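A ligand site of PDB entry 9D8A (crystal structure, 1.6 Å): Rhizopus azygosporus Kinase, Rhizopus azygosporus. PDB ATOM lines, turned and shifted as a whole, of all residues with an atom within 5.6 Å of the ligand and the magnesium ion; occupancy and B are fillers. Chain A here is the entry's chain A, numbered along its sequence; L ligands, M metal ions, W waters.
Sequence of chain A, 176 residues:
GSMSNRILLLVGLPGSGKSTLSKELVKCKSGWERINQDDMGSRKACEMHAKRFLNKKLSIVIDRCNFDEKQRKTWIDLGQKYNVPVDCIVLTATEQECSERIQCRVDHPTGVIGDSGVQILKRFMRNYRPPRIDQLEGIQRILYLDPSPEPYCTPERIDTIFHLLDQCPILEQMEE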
ATOM      1  N   LEU A  13      -1.970  22.942 -32.672  1.00  0.00           N
ATOM      2  CA  LEU A  13      -2.482  21.595 -32.559  1.00  0.00           C
ATOM      3  C   LEU A  13      -3.346  21.458 -31.308  1.00  0.00           C
ATOM      4  O   LEU A  13      -3.168  22.169 -30.336  1.00  0.00           O
ATOM      5  CB  LEU A  13      -1.290  20.629 -32.479  1.00  0.00           C
ATOM      6  CG  LEU A  13      -0.311  20.641 -33.647  1.00  0.00           C
ATOM      7  CD1 LEU A  13       0.838  19.648 -33.408  1.00  0.00           C
ATOM      8  CD2 LEU A  13      -0.991  20.344 -34.939  1.00  0.00           C
ATOM      9  N   PRO A  14      -4.225  20.441 -31.257  1.00  0.00           N
ATOM     10  CA  PRO A  14      -4.807  20.000 -29.997  1.00  0.00           C
ATOM     11  C   PRO A  14      -3.666  19.738 -29.010  1.00  0.00           C
ATOM     12  O   PRO A  14      -2.658  19.108 -29.388  1.00  0.00           O
ATOM     13  CB  PRO A  14      -5.528  18.712 -30.417  1.00  0.00           C
ATOM     14  CG  PRO A  14      -5.783  18.831 -31.872  1.00  0.00           C
ATOM     15  CD  PRO A  14      -4.631  19.627 -32.395  1.00  0.00           C
ATOM     16  N   GLY A  15      -3.802  20.254 -27.800  1.00  0.00           N
ATOM     17  CA  GLY A  15      -2.833  20.073 -26.720  1.00  0.00           C
ATOM     18  C   GLY A  15      -1.656  21.056 -26.759  1.00  0.00           C
ATOM     19  O   GLY A  15      -0.776  21.035 -25.901  1.00  0.00           O
ATOM     20  N   SER A  16      -1.692  22.032 -27.690  1.00  0.00           N
ATOM     21  CA  SER A  16      -0.578  22.933 -27.862  1.00  0.00           C
ATOM     22  C   SER A  16      -0.559  24.056 -26.834  1.00  0.00           C
ATOM     23  O   SER A  16       0.493  24.674 -26.664  1.00  0.00           O
ATOM     24  CB  SER A  16      -0.529  23.509 -29.279  1.00  0.00           C
ATOM     25  OG  SER A  16      -1.676  24.284 -29.568  1.00  0.00           O
ATOM     26  N   GLY A  17      -1.697  24.358 -26.199  1.00  0.00           N
ATOM     27  CA  GLY A  17      -1.732  25.337 -25.133  1.00  0.00           C
ATOM     28  C   GLY A  17      -2.638  26.531 -25.411  1.00  0.00           C
ATOM     29  O   GLY A  17      -2.509  27.574 -24.761  1.00  0.00           O
ATOM     30  N   LYS A  18      -3.593  26.365 -26.338  1.00  0.00           N
ATOM     31  CA  LYS A  18      -4.464  27.476 -26.706  1.00  0.00           C
ATOM     32  C   LYS A  18      -5.359  27.923 -25.559  1.00  0.00           C
ATOM     33  O   LYS A  18      -5.482  29.122 -25.297  1.00  0.00           O
ATOM     34  CB  LYS A  18      -5.317  27.063 -27.908  1.00  0.00           C
ATOM     35  CG  LYS A  18      -4.521  26.766 -29.135  1.00  0.00           C
ATOM     36  CD  LYS A  18      -5.410  26.298 -30.284  1.00  0.00           C
ATOM     37  CE  LYS A  18      -6.375  25.165 -29.992  1.00  0.00           C
ATOM     38  NZ  LYS A  18      -5.648  23.894 -29.842  1.00  0.00           N
ATOM     39  N   SER A  19      -6.031  26.969 -24.894  1.00  0.00           N
ATOM     40  CA  SER A  19      -6.903  27.286 -23.769  1.00  0.00           C
ATOM     41  C   SER A  19      -6.116  27.839 -22.576  1.00  0.00           C
ATOM     42  O   SER A  19      -6.595  28.742 -21.891  1.00  0.00           O
ATOM     43  CB  SER A  19      -7.763  26.092 -23.343  1.00  0.00           C
ATOM     44  OG  SER A  19      -8.514  25.586 -24.447  1.00  0.00           O
ATOM     45  N   THR A  20      -4.916  27.303 -22.326  1.00  0.00           N
ATOM     46  CA  THR A  20      -4.062  27.794 -21.246  1.00  0.00           C
ATOM     47  C   THR A  20      -3.795  29.277 -21.440  1.00  0.00           C
ATOM     48  O   THR A  20      -3.957  30.068 -20.516  1.00  0.00           O
ATOM     49  CB  THR A  20      -2.761  26.987 -21.183  1.00  0.00           C
ATOM     50  OG1 THR A  20      -3.107  25.622 -20.951  1.00  0.00           O
ATOM     51  CG2 THR A  20      -1.836  27.444 -20.066  1.00  0.00           C
ATOM     52  N   LEU A  21      -3.380  29.667 -22.652  1.00  0.00           N
ATOM     53  CA  LEU A  21      -3.087  31.064 -22.933  1.00  0.00           C
ATOM     54  C   LEU A  21      -4.359  31.915 -22.825  1.00  0.00           C
ATOM     55  O   LEU A  21      -4.370  32.961 -22.176  1.00  0.00           O
ATOM     56  CB  LEU A  21      -2.448  31.125 -24.320  1.00  0.00           C
ATOM     57  CG  LEU A  21      -1.814  32.445 -24.768  1.00  0.00           C
ATOM     58  CD1 LEU A  21      -0.932  32.274 -26.006  1.00  0.00           C
ATOM     59  CD2 LEU A  21      -2.903  33.431 -25.099  1.00  0.00           C
ATOM     60  N   ARG A  34     -13.204  35.348 -24.468  1.00  0.00           N
ATOM     61  CA  ARG A  34     -12.710  34.151 -25.101  1.00  0.00           C
ATOM     62  C   ARG A  34     -13.863  33.547 -25.868  1.00  0.00           C
ATOM     63  O   ARG A  34     -14.951  33.455 -25.323  1.00  0.00           O
ATOM     64  CB  ARG A  34     -12.164  33.235 -23.980  1.00  0.00           C
ATOM     65  CG  ARG A  34     -11.699  31.865 -24.408  1.00  0.00           C
ATOM     66  CD  ARG A  34     -11.157  31.128 -23.164  1.00  0.00           C
ATOM     67  NE  ARG A  34     -10.994  29.716 -23.525  1.00  0.00           N
ATOM     68  CZ  ARG A  34     -11.816  28.741 -23.171  1.00  0.00           C
ATOM     69  NH1 ARG A  34     -12.840  28.956 -22.354  1.00  0.00           N
ATOM     70  NH2 ARG A  34     -11.601  27.536 -23.676  1.00  0.00           N
ATOM     71  N   ASN A  36     -14.851  30.078 -27.651  1.00  0.00           N
ATOM     72  CA  ASN A  36     -14.444  28.665 -27.612  1.00  0.00           C
ATOM     73  C   ASN A  36     -15.619  27.737 -27.926  1.00  0.00           C
ATOM     74  O   ASN A  36     -16.597  27.782 -27.192  1.00  0.00           O
ATOM     75  CB  ASN A  36     -13.964  28.243 -26.236  1.00  0.00           C
ATOM     76  CG  ASN A  36     -13.601  26.776 -26.238  1.00  0.00           C
ATOM     77  OD1 ASN A  36     -14.311  25.959 -25.635  1.00  0.00           O
ATOM     78  ND2 ASN A  36     -12.558  26.426 -26.981  1.00  0.00           N
ATOM     79  N   ASP A  63     -10.067  30.774 -29.417  1.00  0.00           N
ATOM     80  CA  ASP A  63      -9.422  29.605 -28.844  1.00  0.00           C
ATOM     81  C   ASP A  63     -10.039  28.397 -29.542  1.00  0.00           C
ATOM     82  O   ASP A  63     -11.004  27.804 -29.026  1.00  0.00           O
ATOM     83  CB  ASP A  63      -9.657  29.512 -27.336  1.00  0.00           C
ATOM     84  CG  ASP A  63      -9.153  28.221 -26.683  1.00  0.00           C
ATOM     85  OD1 ASP A  63      -8.411  27.481 -27.364  1.00  0.00           O
ATOM     86  OD2 ASP A  63      -9.516  27.938 -25.502  1.00  0.00           O
ATOM     87  N   LEU A  91       1.107  28.639 -31.907  1.00  0.00           N
ATOM     88  CA  LEU A  91       1.798  27.935 -30.825  1.00  0.00           C
ATOM     89  C   LEU A  91       2.665  26.871 -31.504  1.00  0.00           C
ATOM     90  O   LEU A  91       2.157  26.100 -32.298  1.00  0.00           O
ATOM     91  CB  LEU A  91       0.758  27.335 -29.873  1.00  0.00           C
ATOM     92  CG  LEU A  91      -0.050  28.310 -29.018  1.00  0.00           C
ATOM     93  CD1 LEU A  91      -0.792  27.638 -27.901  1.00  0.00           C
ATOM     94  CD2 LEU A  91       0.735  29.462 -28.448  1.00  0.00           C
ATOM     95  N   ARG A 101       1.400  15.512 -24.002  1.00  0.00           N
ATOM     96  CA  ARG A 101       0.473  16.218 -23.141  1.00  0.00           C
ATOM     97  C   ARG A 101      -0.912  15.571 -23.160  1.00  0.00           C
ATOM     98  O   ARG A 101      -1.528  15.482 -22.121  1.00  0.00           O
ATOM     99  CB  ARG A 101       0.395  17.684 -23.550  1.00  0.00           C
ATOM    100  CG  ARG A 101       1.688  18.487 -23.472  1.00  0.00           C
ATOM    101  CD  ARG A 101       1.550  19.788 -24.249  1.00  0.00           C
ATOM    102  NE  ARG A 101       2.744  20.627 -24.191  1.00  0.00           N
ATOM    103  CZ  ARG A 101       2.802  21.856 -24.714  1.00  0.00           C
ATOM    104  NH1 ARG A 101       1.687  22.383 -25.190  1.00  0.00           N
ATOM    105  NH2 ARG A 101       3.909  22.576 -24.717  1.00  0.00           N
ATOM    106  N   ARG A 105      -4.018  13.582 -20.327  1.00  0.00           N
ATOM    107  CA  ARG A 105      -5.392  13.925 -19.996  1.00  0.00           C
ATOM    108  C   ARG A 105      -6.191  12.670 -19.628  1.00  0.00           C
ATOM    109  O   ARG A 105      -6.115  11.663 -20.316  1.00  0.00           O
ATOM    110  CB  ARG A 105      -6.047  14.566 -21.225  1.00  0.00           C
ATOM    111  CG  ARG A 105      -5.472  15.931 -21.586  1.00  0.00           C
ATOM    112  CD  ARG A 105      -6.084  16.389 -22.913  1.00  0.00           C
ATOM    113  NE  ARG A 105      -5.728  17.777 -23.206  1.00  0.00           N
ATOM    114  CZ  ARG A 105      -6.052  18.413 -24.358  1.00  0.00           C
ATOM    115  NH1 ARG A 105      -6.615  17.761 -25.329  1.00  0.00           N
ATOM    116  NH2 ARG A 105      -5.758  19.711 -24.527  1.00  0.00           N
ATOM    117  N   HIS A 108     -11.616  15.475 -21.031  1.00  0.00           N
ATOM    118  CA  HIS A 108     -11.416  16.796 -21.620  1.00  0.00           C
ATOM    119  C   HIS A 108     -12.656  17.191 -22.407  1.00  0.00           C
ATOM    120  O   HIS A 108     -13.283  16.340 -23.014  1.00  0.00           O
ATOM    121  CB  HIS A 108     -10.229  16.782 -22.601  1.00  0.00           C
ATOM    122  CG  HIS A 108      -9.670  18.150 -22.830  1.00  0.00           C
ATOM    123  ND1 HIS A 108     -10.036  18.910 -23.926  1.00  0.00           N
ATOM    124  CD2 HIS A 108      -8.843  18.900 -22.089  1.00  0.00           C
ATOM    125  CE1 HIS A 108      -9.428  20.077 -23.842  1.00  0.00           C
ATOM    126  NE2 HIS A 108      -8.684  20.096 -22.726  1.00  0.00           N
ATOM    127  N   THR A 110     -12.987  18.466 -25.236  1.00  0.00           N
ATOM    128  CA  THR A 110     -12.846  18.171 -26.664  1.00  0.00           C
ATOM    129  C   THR A 110     -12.952  16.689 -26.978  1.00  0.00           C
ATOM    130  O   THR A 110     -13.065  16.302 -28.142  1.00  0.00           O
ATOM    131  CB  THR A 110     -11.521  18.683 -27.212  1.00  0.00           C
ATOM    132  OG1 THR A 110     -10.441  18.007 -26.564  1.00  0.00           O
ATOM    133  CG2 THR A 110     -11.377  20.189 -27.042  1.00  0.00           C
ATOM    134  N   ASP A 146       7.099  30.132 -28.813  1.00  0.00           N
ATOM    135  CA  ASP A 146       7.711  28.912 -28.285  1.00  0.00           C
ATOM    136  C   ASP A 146       7.002  28.536 -26.975  1.00  0.00           C
ATOM    137  O   ASP A 146       6.594  29.415 -26.209  1.00  0.00           O
ATOM    138  CB  ASP A 146       9.182  29.108 -27.977  1.00  0.00           C
ATOM    139  CG  ASP A 146      10.137  29.198 -29.170  1.00  0.00           C
ATOM    140  OD1 ASP A 146       9.758  28.797 -30.270  1.00  0.00           O
ATOM    141  OD2 ASP A 146      11.252  29.665 -28.969  1.00  0.00           O
ATOM    142  N   PRO A 147       6.904  27.215 -26.660  1.00  0.00           N
ATOM    143  CA  PRO A 147       6.419  26.760 -25.372  1.00  0.00           C
ATOM    144  C   PRO A 147       7.305  27.296 -24.254  1.00  0.00           C
ATOM    145  O   PRO A 147       8.521  27.367 -24.410  1.00  0.00           O
ATOM    146  CB  PRO A 147       6.493  25.218 -25.439  1.00  0.00           C
ATOM    147  CG  PRO A 147       6.731  24.875 -26.863  1.00  0.00           C
ATOM    148  CD  PRO A 147       7.341  26.115 -27.530  1.00  0.00           C
ATOM    149  N   SER A 148       6.694  27.609 -23.112  1.00  0.00           N
ATOM    150  CA  SER A 148       7.442  27.803 -21.884  1.00  0.00           C
ATOM    151  C   SER A 148       7.853  26.446 -21.310  1.00  0.00           C
ATOM    152  O   SER A 148       7.203  25.435 -21.565  1.00  0.00           O
ATOM    153  CB  SER A 148       6.635  28.550 -20.872  1.00  0.00           C
ATOM    154  OG  SER A 148       5.489  27.791 -20.592  1.00  0.00           O
ATOM    155  N   PRO A 149       8.928  26.388 -20.506  1.00  0.00           N
ATOM    156  CA  PRO A 149       9.274  25.185 -19.741  1.00  0.00           C
ATOM    157  C   PRO A 149       8.143  24.730 -18.812  1.00  0.00           C
ATOM    158  O   PRO A 149       7.921  23.527 -18.653  1.00  0.00           O
ATOM    159  CB  PRO A 149      10.574  25.557 -18.973  1.00  0.00           C
ATOM    160  CG  PRO A 149      11.021  26.908 -19.495  1.00  0.00           C
ATOM    161  CD  PRO A 149       9.895  27.490 -20.334  1.00  0.00           C
ATOM    162  N   GLU A 150       7.435  25.695 -18.210  1.00  0.00           N
ATOM    163  CA  GLU A 150       6.364  25.480 -17.256  1.00  0.00           C
ATOM    164  C   GLU A 150       5.018  25.272 -17.949  1.00  0.00           C
ATOM    165  O   GLU A 150       4.770  25.852 -18.994  1.00  0.00           O
ATOM    166  CB  GLU A 150       6.118  26.735 -16.420  1.00  0.00           C
ATOM    167  CG  GLU A 150       7.246  27.051 -15.440  1.00  0.00           C
ATOM    168  CD  GLU A 150       8.458  27.699 -16.094  1.00  0.00           C
ATOM    169  OE1 GLU A 150       8.303  28.323 -17.187  1.00  0.00           O
ATOM    170  OE2 GLU A 150       9.547  27.544 -15.499  1.00  0.00           O
ATOM    171  N   PRO A 151       4.122  24.452 -17.364  1.00  0.00           N
ATOM    172  CA  PRO A 151       2.823  24.118 -17.953  1.00  0.00           C
ATOM    173  C   PRO A 151       1.692  25.119 -17.723  1.00  0.00           C
ATOM    174  O   PRO A 151       0.622  25.025 -18.330  1.00  0.00           O
ATOM    175  CB  PRO A 151       2.530  22.737 -17.368  1.00  0.00           C
ATOM    176  CG  PRO A 151       3.242  22.726 -16.052  1.00  0.00           C
ATOM    177  CD  PRO A 151       4.430  23.643 -16.180  1.00  0.00           C
ATOM    178  N   TYR A 152       1.975  26.154 -16.950  1.00  0.00           N
ATOM    179  CA  TYR A 152       0.970  27.145 -16.618  1.00  0.00           C
ATOM    180  C   TYR A 152       1.388  28.462 -17.266  1.00  0.00           C
ATOM    181  O   TYR A 152       2.553  28.648 -17.622  1.00  0.00           O
ATOM    182  CB  TYR A 152       0.906  27.206 -15.101  1.00  0.00           C
ATOM    183  CG  TYR A 152       2.231  27.487 -14.390  1.00  0.00           C
ATOM    184  CD1 TYR A 152       2.708  28.784 -14.258  1.00  0.00           C
ATOM    185  CD2 TYR A 152       2.967  26.450 -13.807  1.00  0.00           C
ATOM    186  CE1 TYR A 152       3.887  29.049 -13.585  1.00  0.00           C
ATOM    187  CE2 TYR A 152       4.164  26.707 -13.154  1.00  0.00           C
ATOM    188  CZ  TYR A 152       4.615  28.014 -13.029  1.00  0.00           C
ATOM    189  OH  TYR A 152       5.795  28.283 -12.386  1.00  0.00           O
ATOM    190  N   ARG A 157       3.855  36.124 -18.334  1.00  0.00           N
ATOM    191  CA  ARG A 157       3.952  35.534 -19.663  1.00  0.00           C
ATOM    192  C   ARG A 157       3.002  36.250 -20.636  1.00  0.00           C
ATOM    193  O   ARG A 157       3.358  36.486 -21.803  1.00  0.00           O
ATOM    194  CB  ARG A 157       3.637  34.039 -19.640  1.00  0.00           C
ATOM    195  CG  ARG A 157       3.725  33.442 -21.040  1.00  0.00           C
ATOM    196  CD  ARG A 157       3.888  31.942 -20.955  1.00  0.00           C
ATOM    197  NE  ARG A 157       3.845  31.209 -22.212  1.00  0.00           N
ATOM    198  CZ  ARG A 157       4.800  31.100 -23.114  1.00  0.00           C
ATOM    199  NH1 ARG A 157       5.948  31.704 -22.915  1.00  0.00           N
ATOM    200  NH2 ARG A 157       4.583  30.440 -24.218  1.00  0.00           N
HETATM  201  P1  LIG L   1      -5.299  23.232 -26.154  1.00  0.00           P
HETATM  202  O1  LIG L   1      -4.450  23.795 -27.280  1.00  0.00           O
HETATM  203  O2  LIG L   1      -5.791  21.878 -26.565  1.00  0.00           O
HETATM  204  O3  LIG L   1      -6.385  24.083 -25.547  1.00  0.00           O
HETATM  205  O4  LIG L   1      -4.130  22.974 -25.028  1.00  0.00           O
HETATM  206  P2  LIG L   1      -4.306  23.205 -23.474  1.00  0.00           P
HETATM  207  O5  LIG L   1      -4.365  24.640 -22.958  1.00  0.00           O
HETATM  208  O6  LIG L   1      -5.442  22.332 -22.953  1.00  0.00           O
HETATM  209  O7  LIG L   1      -2.840  22.710 -22.902  1.00  0.00           O
HETATM  210  C1  LIG L   1      -2.465  21.314 -22.993  1.00  0.00           C
HETATM  211  C2  LIG L   1      -1.432  21.036 -21.916  1.00  0.00           C
HETATM  212  O8  LIG L   1      -0.248  21.591 -22.181  1.00  0.00           O
HETATM  213  C3  LIG L   1      -1.901  21.697 -20.493  1.00  0.00           C
HETATM  214  O9  LIG L   1      -1.662  20.689 -19.514  1.00  0.00           O
HETATM  215  C4  LIG L   1      -1.145  22.684 -20.294  1.00  0.00           C
HETATM  216  O10 LIG L   1      -0.760  22.928 -18.887  1.00  0.00           O
HETATM  217  C5  LIG L   1       0.232  22.476 -21.099  1.00  0.00           C
HETATM  218  N1  LIG L   1       0.712  23.648 -21.641  1.00  0.00           N
HETATM  219  C6  LIG L   1       0.072  24.725 -22.228  1.00  0.00           C
HETATM  220  N2  LIG L   1       0.948  25.650 -22.690  1.00  0.00           N
HETATM  221  C7  LIG L   1       2.163  25.195 -22.366  1.00  0.00           C
HETATM  222  C8  LIG L   1       3.553  25.747 -22.583  1.00  0.00           C
HETATM  223  O11 LIG L   1       3.856  26.796 -23.095  1.00  0.00           O
HETATM  224  N3  LIG L   1       4.639  24.955 -22.114  1.00  0.00           N
HETATM  225  C9  LIG L   1       4.417  23.707 -21.439  1.00  0.00           C
HETATM  226  N4  LIG L   1       5.561  23.010 -20.952  1.00  0.00           N
HETATM  227  N5  LIG L   1       3.124  23.168 -21.243  1.00  0.00           N
HETATM  228  C10 LIG L   1       1.972  23.943 -21.730  1.00  0.00           C
HETATM  229 MG    MG M   1      -8.418  23.826 -25.415  1.00  0.00          MG
HETATM  230  O   HOH W   1       2.606  28.235 -20.436  1.00  0.00           O
HETATM  231  O   HOH W   2      -8.697  24.996 -27.112  1.00  0.00           O
HETATM  232  O   HOH W   3      -8.154  22.812 -23.652  1.00  0.00           O
HETATM  233  O   HOH W   4      -4.811  19.496 -21.045  1.00  0.00           O
HETATM  234  O   HOH W   5     -10.434  23.640 -25.172  1.00  0.00           O
HETATM  235  O   HOH W   6      -3.681  24.519 -18.511  1.00  0.00           O
HETATM  236  O   HOH W   7      -0.007  28.097 -23.806  1.00  0.00           O
HETATM  237  O   HOH W   8      -8.310  22.129 -26.478  1.00  0.00           O
HETATM  238  O   HOH W   9       2.635  28.430 -24.939  1.00  0.00           O
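Water W3 bridges an oxygen (O6) of the ligand (2.8 Å) and a ring nitrogen (NE2) of His 108 (2.9 Å).
Water W9 lies within hydrogen-bond range of an oxygen (O11) of the ligand (2.7 Å) and the guanidinium group of Arg 157 (2.9 Å).
Water W7 lies within hydrogen-bond range of the backbone carbonyl oxygen (O) of Gly 17 (2.7 Å) and a nitrogen (N2) of the ligand (2.9 Å).
Water W1 lies within hydrogen-bond range of the backbone carbonyl oxygen of Tyr 152 (2.8 Å), the side-chain hydroxyl of Ser 148 (2.9 Å) and an oxygen (O11) of the ligand (3.3 Å).
Water W6 bridges the side-chain hydroxyl (OG1) of Thr 20 (2.7 Å) and an oxygen (O10) of the ligand (3.3 Å).
Water W4 lies within hydrogen-bond range of NE of Arg 105 and O6 of the ligand.
An oxygen (O5) of the ligand lies within hydrogen-bond range of the backbone NH (N) of Ser 19, 3.5 Å away.
The backbone NH of Thr 20 lies within hydrogen-bond range of an oxygen (O5) of the ligand.
OG1 of Thr 20 is in hydrogen-bond range of O5 of the ligand, 2.6 Å away.
The backbone carbonyl oxygen of Pro 151 lies within hydrogen-bond range of an oxygen (O10) of the ligand, at 2.6 Å.
The backbone NH (N) of Ser 148 lies within hydrogen-bond range of an oxygen (O11) of the ligand (3.0 Å).
O of Ser 148 is in hydrogen-bond range of N3 of the ligand, 2.7 Å away.
O11 of the ligand lies within hydrogen-bond range of OG of Ser 148 (3.1 Å).
The backbone NH (N) of Lys 18 sits at hydrogen-bond distance from an oxygen (O1) of the ligand.
NZ of Lys 18 lies within salt-bridge range of O1 of the ligand, 2.8 Å away.
N of Gly 15 is in hydrogen-bond range of O2 of the ligand, at 2.8 Å.
The guanidinium group of Arg 105 lies within salt-bridge range of an oxygen (O2) of the ligand, at 3.0 Å.
An oxygen (O1) of the ligand lies within hydrogen-bond range of the backbone NH (N) of Gly 17, 3.0 Å away.
The backbone carbonyl oxygen of Glu 150 is in hydrogen-bond range of a nitrogen (N3) of the ligand (3.2 Å).
An oxygen (O1) of the ligand is in hydrogen-bond range of the backbone NH (N) of Ser 16 (3.3 Å).
O of Pro 149 sits at hydrogen-bond distance from N4 of the ligand (3.3 Å).
The backbone carbonyl oxygen (O) of Glu 150 is in hydrogen-bond range of the side-chain hydroxyl (OG) of Ser 148, 2.6 Å away.
NZ of Lys 18 sits at hydrogen-bond distance from O of Leu 13.
The backbone carbonyl oxygen (O) of Gly 15 is in hydrogen-bond range of the guanidinium group (NH1) of Arg 101 (2.9 Å).
NE2 of His 108 lies within hydrogen-bond range of NH2 of Arg 105 (3.5 Å).
The guanidinium group (NH1) of Arg 101 is in hydrogen-bond range of the backbone carbonyl oxygen (O) of Ser 16, at 3.0 Å.
The side-chain hydroxyl (OG) of Ser 16 is in hydrogen-bond range of the backbone carbonyl oxygen (O) of Leu 13 (2.7 Å).
The guanidinium group of Arg 157 lies within hydrogen-bond range of the backbone carbonyl oxygen of Asp 146 (3.0 Å).
ND1 of His 108 lies within hydrogen-bond range of OG1 of Thr 110 (2.8 Å).
Leu 13 touches the ligand.
C of Pro 14 touches O2 of the ligand, at 3.9 Å.
Arg 101 touches the ligand (CD to O8, 3.3 Å).
His 108 touches the ligand (NE2 to O6, 3.9 Å).
CA of Pro 147 touches O11 of the ligand, 3.4 Å away.
Arg 157 touches the ligand.
Hydrophobic or aromatic side chains that line the ligand: Pro 147 and Pro 151.
Of the 25 residues printed, 17 come within 4 Å of the ligand.
The nearest printed residue that does not touch the ligand is Asp 63 (4.4 Å).
One residue has an atom within 4 Å of the magnesium ion: Ser 19.
The nearest printed residue that does not touch the magnesium ion is Asp 63 (4.1 Å).
The magnesium ion is bound by water W8, the side-chain hydroxyl (OG) of Ser 19, water W5, water W3, an oxygen (O3) of the ligand and water W2.
The magnesium ion has six donor atoms within binding distance.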
